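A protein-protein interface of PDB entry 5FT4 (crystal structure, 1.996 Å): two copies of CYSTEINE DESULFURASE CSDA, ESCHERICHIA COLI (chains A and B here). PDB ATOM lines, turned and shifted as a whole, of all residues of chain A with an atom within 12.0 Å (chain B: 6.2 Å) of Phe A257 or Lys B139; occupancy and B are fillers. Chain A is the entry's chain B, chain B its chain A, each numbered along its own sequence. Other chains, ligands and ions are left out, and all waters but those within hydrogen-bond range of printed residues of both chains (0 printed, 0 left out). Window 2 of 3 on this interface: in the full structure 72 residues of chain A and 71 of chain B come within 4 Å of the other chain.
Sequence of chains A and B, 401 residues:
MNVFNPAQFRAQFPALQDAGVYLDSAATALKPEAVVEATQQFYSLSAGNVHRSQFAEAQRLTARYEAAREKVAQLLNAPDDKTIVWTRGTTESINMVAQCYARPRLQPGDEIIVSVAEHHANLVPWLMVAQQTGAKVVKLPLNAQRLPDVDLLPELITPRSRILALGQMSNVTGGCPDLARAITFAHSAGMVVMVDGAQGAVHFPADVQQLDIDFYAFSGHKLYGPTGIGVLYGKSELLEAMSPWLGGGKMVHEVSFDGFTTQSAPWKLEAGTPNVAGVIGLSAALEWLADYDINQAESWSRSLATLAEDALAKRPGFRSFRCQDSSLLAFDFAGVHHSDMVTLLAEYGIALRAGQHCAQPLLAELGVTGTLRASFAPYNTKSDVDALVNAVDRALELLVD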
ATOM      1  N   VAL A 252      19.977  17.422  16.644  1.00  0.00           N
ATOM      2  CA  VAL A 252      18.680  16.832  16.297  1.00  0.00           C
ATOM      3  C   VAL A 252      17.719  17.889  15.850  1.00  0.00           C
ATOM      4  O   VAL A 252      17.927  19.103  16.090  1.00  0.00           O
ATOM      5  CB  VAL A 252      17.921  16.058  17.425  1.00  0.00           C
ATOM      6  CG1 VAL A 252      18.607  14.797  17.796  1.00  0.00           C
ATOM      7  CG2 VAL A 252      17.583  16.970  18.645  1.00  0.00           C
ATOM      8  N   HIS A 253      16.715  17.418  15.115  1.00  0.00           N
ATOM      9  CA  HIS A 253      15.592  18.250  14.763  1.00  0.00           C
ATOM     10  C   HIS A 253      14.295  17.729  15.417  1.00  0.00           C
ATOM     11  O   HIS A 253      13.828  18.300  16.413  1.00  0.00           O
ATOM     12  CB  HIS A 253      15.449  18.349  13.239  1.00  0.00           C
ATOM     13  CG  HIS A 253      14.474  19.406  12.815  1.00  0.00           C
ATOM     14  ND1 HIS A 253      13.669  19.288  11.708  1.00  0.00           N
ATOM     15  CD2 HIS A 253      14.192  20.615  13.355  1.00  0.00           C
ATOM     16  CE1 HIS A 253      12.908  20.361  11.598  1.00  0.00           C
ATOM     17  NE2 HIS A 253      13.211  21.185  12.582  1.00  0.00           N
ATOM     18  N   GLU A 254      13.692  16.671  14.875  1.00  0.00           N
ATOM     19  CA  GLU A 254      12.483  16.103  15.497  1.00  0.00           C
ATOM     20  C   GLU A 254      12.946  14.961  16.393  1.00  0.00           C
ATOM     21  O   GLU A 254      13.884  14.250  16.023  1.00  0.00           O
ATOM     22  CB  GLU A 254      11.504  15.561  14.432  1.00  0.00           C
ATOM     23  CG  GLU A 254      11.044  16.567  13.400  1.00  0.00           C
ATOM     24  CD  GLU A 254      10.047  17.556  13.953  1.00  0.00           C
ATOM     25  OE1 GLU A 254       9.406  17.228  14.965  1.00  0.00           O
ATOM     26  OE2 GLU A 254       9.896  18.653  13.378  1.00  0.00           O
ATOM     27  N   VAL A 255      12.314  14.799  17.557  1.00  0.00           N
ATOM     28  CA  VAL A 255      12.625  13.702  18.472  1.00  0.00           C
ATOM     29  C   VAL A 255      11.360  13.185  19.124  1.00  0.00           C
ATOM     30  O   VAL A 255      10.569  13.974  19.612  1.00  0.00           O
ATOM     31  CB  VAL A 255      13.578  14.131  19.641  1.00  0.00           C
ATOM     32  CG1 VAL A 255      13.857  12.951  20.579  1.00  0.00           C
ATOM     33  CG2 VAL A 255      14.873  14.716  19.134  1.00  0.00           C
ATOM     34  N   SER A 256      11.215  11.865  19.147  1.00  0.00           N
ATOM     35  CA  SER A 256      10.175  11.167  19.921  1.00  0.00           C
ATOM     36  C   SER A 256      10.799   9.912  20.503  1.00  0.00           C
ATOM     37  O   SER A 256      11.962   9.631  20.255  1.00  0.00           O
ATOM     38  CB  SER A 256       8.963  10.766  19.064  1.00  0.00           C
ATOM     39  OG  SER A 256       9.245   9.592  18.320  1.00  0.00           O
ATOM     40  N   PHE A 257      10.030   9.140  21.260  1.00  0.00           N
ATOM     41  CA  PHE A 257      10.545   7.895  21.827  1.00  0.00           C
ATOM     42  C   PHE A 257      10.627   6.790  20.785  1.00  0.00           C
ATOM     43  O   PHE A 257      11.163   5.725  21.063  1.00  0.00           O
ATOM     44  CB  PHE A 257       9.679   7.488  23.034  1.00  0.00           C
ATOM     45  CG  PHE A 257      10.212   8.030  24.330  1.00  0.00           C
ATOM     46  CD1 PHE A 257      10.045   9.366  24.670  1.00  0.00           C
ATOM     47  CD2 PHE A 257      10.954   7.213  25.186  1.00  0.00           C
ATOM     48  CE1 PHE A 257      10.603   9.858  25.849  1.00  0.00           C
ATOM     49  CE2 PHE A 257      11.503   7.708  26.355  1.00  0.00           C
ATOM     50  CZ  PHE A 257      11.327   9.025  26.691  1.00  0.00           C
ATOM     51  N   ASP A 258      10.132   7.069  19.578  1.00  0.00           N
ATOM     52  CA  ASP A 258      10.257   6.158  18.439  1.00  0.00           C
ATOM     53  C   ASP A 258      11.486   6.407  17.555  1.00  0.00           C
ATOM     54  O   ASP A 258      11.932   5.513  16.842  1.00  0.00           O
ATOM     55  CB  ASP A 258       8.992   6.223  17.593  1.00  0.00           C
ATOM     56  CG  ASP A 258       7.797   5.656  18.324  1.00  0.00           C
ATOM     57  OD1 ASP A 258       7.987   4.636  19.012  1.00  0.00           O
ATOM     58  OD2 ASP A 258       6.691   6.227  18.225  1.00  0.00           O
ATOM     59  N   GLY A 259      12.052   7.602  17.609  1.00  0.00           N
ATOM     60  CA  GLY A 259      13.202   7.896  16.773  1.00  0.00           C
ATOM     61  C   GLY A 259      13.433   9.379  16.563  1.00  0.00           C
ATOM     62  O   GLY A 259      12.812  10.208  17.243  1.00  0.00           O
ATOM     63  N   PHE A 260      14.319   9.729  15.631  1.00  0.00           N
ATOM     64  CA  PHE A 260      14.689  11.146  15.480  1.00  0.00           C
ATOM     65  C   PHE A 260      15.151  11.475  14.088  1.00  0.00           C
ATOM     66  O   PHE A 260      15.494  10.600  13.316  1.00  0.00           O
ATOM     67  CB  PHE A 260      15.792  11.517  16.467  1.00  0.00           C
ATOM     68  CG  PHE A 260      17.079  10.779  16.230  1.00  0.00           C
ATOM     69  CD1 PHE A 260      17.257   9.508  16.738  1.00  0.00           C
ATOM     70  CD2 PHE A 260      18.117  11.362  15.488  1.00  0.00           C
ATOM     71  CE1 PHE A 260      18.453   8.803  16.507  1.00  0.00           C
ATOM     72  CE2 PHE A 260      19.315  10.681  15.285  1.00  0.00           C
ATOM     73  CZ  PHE A 260      19.476   9.395  15.780  1.00  0.00           C
ATOM     74  N   THR A 261      15.127  12.754  13.774  1.00  0.00           N
ATOM     75  CA  THR A 261      15.760  13.280  12.587  1.00  0.00           C
ATOM     76  C   THR A 261      16.832  14.275  13.044  1.00  0.00           C
ATOM     77  O   THR A 261      16.818  14.729  14.176  1.00  0.00           O
ATOM     78  CB  THR A 261      14.761  13.985  11.672  1.00  0.00           C
ATOM     79  OG1 THR A 261      14.229  15.138  12.341  1.00  0.00           O
ATOM     80  CG2 THR A 261      13.649  13.032  11.265  1.00  0.00           C
ATOM     81  N   ILE B 112      16.009  -0.327  27.641  1.00  0.00           N
ATOM     82  CA  ILE B 112      16.598   0.875  28.212  1.00  0.00           C
ATOM     83  C   ILE B 112      15.432   1.740  28.643  1.00  0.00           C
ATOM     84  O   ILE B 112      14.685   2.235  27.797  1.00  0.00           O
ATOM     85  CB  ILE B 112      17.452   1.662  27.196  1.00  0.00           C
ATOM     86  CG1 ILE B 112      18.540   0.777  26.555  1.00  0.00           C
ATOM     87  CG2 ILE B 112      18.083   2.883  27.865  1.00  0.00           C
ATOM     88  CD1 ILE B 112      19.084   1.341  25.197  1.00  0.00           C
ATOM     89  N   ILE B 113      15.258   1.906  29.947  1.00  0.00           N
ATOM     90  CA  ILE B 113      14.190   2.747  30.443  1.00  0.00           C
ATOM     91  C   ILE B 113      14.686   4.209  30.479  1.00  0.00           C
ATOM     92  O   ILE B 113      15.697   4.513  31.106  1.00  0.00           O
ATOM     93  CB  ILE B 113      13.688   2.304  31.817  1.00  0.00           C
ATOM     94  CG1 ILE B 113      13.272   0.829  31.780  1.00  0.00           C
ATOM     95  CG2 ILE B 113      12.541   3.196  32.258  1.00  0.00           C
ATOM     96  CD1 ILE B 113      12.702   0.305  33.094  1.00  0.00           C
ATOM     97  N   VAL B 114      13.955   5.091  29.806  1.00  0.00           N
ATOM     98  CA  VAL B 114      14.298   6.524  29.717  1.00  0.00           C
ATOM     99  C   VAL B 114      13.118   7.395  30.160  1.00  0.00           C
ATOM    100  O   VAL B 114      11.975   7.183  29.729  1.00  0.00           O
ATOM    101  CB  VAL B 114      14.686   6.934  28.287  1.00  0.00           C
ATOM    102  CG1 VAL B 114      15.100   8.435  28.224  1.00  0.00           C
ATOM    103  CG2 VAL B 114      15.806   6.034  27.755  1.00  0.00           C
ATOM    104  N   SER B 115      13.377   8.347  31.046  1.00  0.00           N
ATOM    105  CA  SER B 115      12.305   9.226  31.514  1.00  0.00           C
ATOM    106  C   SER B 115      11.823  10.175  30.411  1.00  0.00           C
ATOM    107  O   SER B 115      12.610  10.707  29.649  1.00  0.00           O
ATOM    108  CB  SER B 115      12.772  10.015  32.729  1.00  0.00           C
ATOM    109  OG  SER B 115      12.334  11.352  32.683  1.00  0.00           O
ATOM    110  N   VAL B 116      10.515  10.393  30.357  1.00  0.00           N
ATOM    111  CA  VAL B 116       9.919  11.277  29.367  1.00  0.00           C
ATOM    112  C   VAL B 116      10.350  12.728  29.637  1.00  0.00           C
ATOM    113  O   VAL B 116      10.129  13.614  28.807  1.00  0.00           O
ATOM    114  CB  VAL B 116       8.352  11.150  29.349  1.00  0.00           C
ATOM    115  CG1 VAL B 116       7.717  11.983  30.434  1.00  0.00           C
ATOM    116  CG2 VAL B 116       7.790  11.585  28.010  1.00  0.00           C
ATOM    117  N   ALA B 117      10.924  12.959  30.812  1.00  0.00           N
ATOM    118  CA  ALA B 117      11.372  14.285  31.212  1.00  0.00           C
ATOM    119  C   ALA B 117      12.808  14.611  30.794  1.00  0.00           C
ATOM    120  O   ALA B 117      13.250  15.729  31.012  1.00  0.00           O
ATOM    121  CB  ALA B 117      11.249  14.428  32.727  1.00  0.00           C
ATOM    122  N   GLU B 118      13.535  13.640  30.227  1.00  0.00           N
ATOM    123  CA  GLU B 118      14.930  13.834  29.823  1.00  0.00           C
ATOM    124  C   GLU B 118      15.163  14.912  28.742  1.00  0.00           C
ATOM    125  O   GLU B 118      14.474  14.985  27.732  1.00  0.00           O
ATOM    126  CB  GLU B 118      15.524  12.512  29.288  1.00  0.00           C
ATOM    127  CG  GLU B 118      15.728  11.398  30.327  1.00  0.00           C
ATOM    128  CD  GLU B 118      16.176  11.903  31.702  1.00  0.00           C
ATOM    129  OE1 GLU B 118      17.299  12.466  31.782  1.00  0.00           O
ATOM    130  OE2 GLU B 118      15.411  11.729  32.693  1.00  0.00           O
ATOM    131  N   LEU B 123      18.500  11.239  25.915  1.00  0.00           N
ATOM    132  CA  LEU B 123      17.511  10.477  25.181  1.00  0.00           C
ATOM    133  C   LEU B 123      18.025   9.999  23.825  1.00  0.00           C
ATOM    134  O   LEU B 123      17.917   8.812  23.510  1.00  0.00           O
ATOM    135  CB  LEU B 123      16.241  11.300  24.951  1.00  0.00           C
ATOM    136  CG  LEU B 123      15.195  10.685  24.012  1.00  0.00           C
ATOM    137  CD1 LEU B 123      14.839   9.262  24.444  1.00  0.00           C
ATOM    138  CD2 LEU B 123      13.916  11.535  23.878  1.00  0.00           C
ATOM    139  N   LEU B 127      18.298   6.128  22.015  1.00  0.00           N
ATOM    140  CA  LEU B 127      17.700   5.781  20.719  1.00  0.00           C
ATOM    141  C   LEU B 127      18.763   5.263  19.727  1.00  0.00           C
ATOM    142  O   LEU B 127      18.541   4.284  19.002  1.00  0.00           O
ATOM    143  CB  LEU B 127      16.981   6.983  20.108  1.00  0.00           C
ATOM    144  CG  LEU B 127      15.737   7.459  20.896  1.00  0.00           C
ATOM    145  CD1 LEU B 127      15.284   8.814  20.392  1.00  0.00           C
ATOM    146  CD2 LEU B 127      14.590   6.462  20.751  1.00  0.00           C
ATOM    147  N   VAL B 137      13.894   1.116  23.593  1.00  0.00           N
ATOM    148  CA  VAL B 137      13.744   2.163  24.598  1.00  0.00           C
ATOM    149  C   VAL B 137      12.324   2.134  25.160  1.00  0.00           C
ATOM    150  O   VAL B 137      11.342   2.102  24.416  1.00  0.00           O
ATOM    151  CB  VAL B 137      14.062   3.545  24.020  1.00  0.00           C
ATOM    152  CG1 VAL B 137      13.718   4.640  25.023  1.00  0.00           C
ATOM    153  CG2 VAL B 137      15.544   3.623  23.588  1.00  0.00           C
ATOM    154  N   VAL B 138      12.234   2.129  26.484  1.00  0.00           N
ATOM    155  CA  VAL B 138      10.968   2.052  27.184  1.00  0.00           C
ATOM    156  C   VAL B 138      10.761   3.375  27.942  1.00  0.00           C
ATOM    157  O   VAL B 138      11.634   3.813  28.692  1.00  0.00           O
ATOM    158  CB  VAL B 138      10.926   0.854  28.167  1.00  0.00           C
ATOM    159  CG1 VAL B 138       9.723   0.940  29.077  1.00  0.00           C
ATOM    160  CG2 VAL B 138      10.941  -0.470  27.411  1.00  0.00           C
ATOM    161  N   LYS B 139       9.601   3.989  27.725  1.00  0.00           N
ATOM    162  CA  LYS B 139       9.257   5.281  28.302  1.00  0.00           C
ATOM    163  C   LYS B 139       8.883   5.165  29.787  1.00  0.00           C
ATOM    164  O   LYS B 139       7.975   4.400  30.158  1.00  0.00           O
ATOM    165  CB  LYS B 139       8.080   5.890  27.526  1.00  0.00           C
ATOM    166  CG  LYS B 139       7.637   7.232  28.042  1.00  0.00           C
ATOM    167  CD  LYS B 139       6.388   7.781  27.342  1.00  0.00           C
ATOM    168  CE  LYS B 139       6.550   8.066  25.863  1.00  0.00           C
ATOM    169  NZ  LYS B 139       5.215   8.363  25.251  1.00  0.00           N
ATOM    170  N   LEU B 140       9.560   5.960  30.618  1.00  0.00           N
ATOM    171  CA  LEU B 140       9.167   6.164  32.005  1.00  0.00           C
ATOM    172  C   LEU B 140       8.322   7.437  32.072  1.00  0.00           C
ATOM    173  O   LEU B 140       8.852   8.534  31.949  1.00  0.00           O
ATOM    174  CB  LEU B 140      10.383   6.275  32.917  1.00  0.00           C
ATOM    175  CG  LEU B 140      10.086   6.659  34.379  1.00  0.00           C
ATOM    176  CD1 LEU B 140       9.210   5.635  35.040  1.00  0.00           C
ATOM    177  CD2 LEU B 140      11.397   6.775  35.149  1.00  0.00           C
ATOM    178  N   PRO B 141       7.004   7.294  32.254  1.00  0.00           N
ATOM    179  CA  PRO B 141       6.150   8.485  32.141  1.00  0.00           C
ATOM    180  C   PRO B 141       6.165   9.416  33.355  1.00  0.00           C
ATOM    181  O   PRO B 141       6.772   9.077  34.365  1.00  0.00           O
ATOM    182  CB  PRO B 141       4.754   7.883  31.945  1.00  0.00           C
ATOM    183  CG  PRO B 141       4.799   6.560  32.617  1.00  0.00           C
ATOM    184  CD  PRO B 141       6.213   6.053  32.429  1.00  0.00           C
ATOM    185  N   LEU B 156       7.395  -1.416  35.021  1.00  0.00           N
ATOM    186  CA  LEU B 156       8.091  -1.216  33.761  1.00  0.00           C
ATOM    187  C   LEU B 156       9.349  -2.075  33.643  1.00  0.00           C
ATOM    188  O   LEU B 156       9.768  -2.409  32.532  1.00  0.00           O
ATOM    189  CB  LEU B 156       8.482   0.262  33.621  1.00  0.00           C
ATOM    190  CG  LEU B 156       7.355   1.270  33.423  1.00  0.00           C
ATOM    191  CD1 LEU B 156       7.918   2.672  33.434  1.00  0.00           C
ATOM    192  CD2 LEU B 156       6.645   0.998  32.113  1.00  0.00           C
ATOM    193  N   PRO B 361       9.744  15.640  24.053  1.00  0.00           N
ATOM    194  CA  PRO B 361       8.804  14.678  24.618  1.00  0.00           C
ATOM    195  C   PRO B 361       8.197  15.224  25.921  1.00  0.00           C
ATOM    196  O   PRO B 361       7.018  15.041  26.138  1.00  0.00           O
ATOM    197  CB  PRO B 361       9.672  13.417  24.848  1.00  0.00           C
ATOM    198  CG  PRO B 361      10.828  13.573  23.927  1.00  0.00           C
ATOM    199  CD  PRO B 361      11.089  15.052  23.875  1.00  0.00           C
ATOM    200  N   GLU B 365       4.049  16.035  26.551  1.00  0.00           N
ATOM    201  CA  GLU B 365       3.240  15.536  27.691  1.00  0.00           C
ATOM    202  C   GLU B 365       2.562  16.710  28.402  1.00  0.00           C
ATOM    203  O   GLU B 365       1.432  16.601  28.898  1.00  0.00           O
ATOM    204  CB  GLU B 365       4.088  14.756  28.718  1.00  0.00           C
ATOM    205  CG  GLU B 365       4.689  13.444  28.227  1.00  0.00           C
ATOM    206  CD  GLU B 365       3.671  12.320  28.059  1.00  0.00           C
ATOM    207  OE1 GLU B 365       2.488  12.528  28.406  1.00  0.00           O
ATOM    208  OE2 GLU B 365       4.064  11.226  27.579  1.00  0.00           O
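The backbone NH (N) of Val B114 lies within hydrogen-bond range of the backbone carbonyl oxygen (O) of Val B138 (2.9 Å). The backbone carbonyl oxygen of Val B114 sits at hydrogen-bond distance from the backbone NH of Leu B140 (2.8 Å). The side-chain hydroxyl (OG) of Ser B115 is in hydrogen-bond range of the backbone NH (N) of Ala B117. The side-chain hydroxyl (OG) of Ser B115 sits at hydrogen-bond distance from the side-chain carboxylate (OE2) of Glu B118 (3.1 Å). The backbone NH of Val B116 sits at hydrogen-bond distance from the backbone carbonyl oxygen of Leu B140 (3.0 Å). The side-chain amino group (NZ) of Lys B139 lies within salt-bridge range of the side-chain carboxylate (OE2) of Glu B365 (3.9 Å).
Among the printed residues, pairs that only touch across the chains: Ser A256 with Leu B127, Phe A257 with Val B114, Phe A257 with Leu B127, Val A255 with Leu B123, Phe A257 with Ser B115, Phe A257 with Val B116, Phe A257 with Val B137, Phe A257 with Pro B361 and Phe A257 with Lys B139.
Of the printed residues of chain B, Val A255 touches Leu B123 (3.6 Å). Printed residues of chain B within 4 Å of Ser A256: Leu B127. Phe A257 touches just these residues of chain B: Val B114, Ser B115, Val B116, Leu B127, Val B137, Lys B139 and Pro B361. No residue of chain A comes within 4 Å of Ile B113. Val B114 touches just one residue of chain A: Phe A257 (3.4 Å). Val B116 touches just one residue of chain A: Phe A257 (3.8 Å). Of the printed residues of chain A, Leu B123 touches Val A255. Leu B127 touches just these residues of chain A: Ser A256 (3.4 Å) and Phe A257 (3.5 Å). No residue of chain A comes within 4 Å of Val B138. Of chain A, only Phe A257 (3.8 Å) comes within 4 Å of Lys B139. No residue of chain A comes within 4 Å of Pro B141. No residue of chain A comes within 4 Å of Leu B156. Of chain A, only Phe A257 comes within 4 Å of Pro B361. The nearest residue of chain B that does not touch Phe A257 is Leu B123 (4.1 Å). The nearest printed residue of chain A that does not touch Leu B123 is Phe A257 (4.1 Å).
Hydrophobic or aromatic side chains of chain B that line the printed part of chain A: Val B114, Val B116, Leu B123, Leu B127, Val B137 and Pro B361. Of the 10 printed residues of chain A, 3 touch a printed residue of chain B. Printed residues of chain A that touch a printed residue of chain B: Val A255, Ser A256 and Phe A257. Hydrophobic or aromatic side chains of chain A within 4 Å of the printed part of chain B: Val A255 and Phe A257. Among the printed residues, 9 pairs touch across the chains. Among the printed residues, no Asp or Glu carboxylate lies within 4 Å of a Lys or Arg side-chain nitrogen of the other chain.
No position is printed for both chains.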
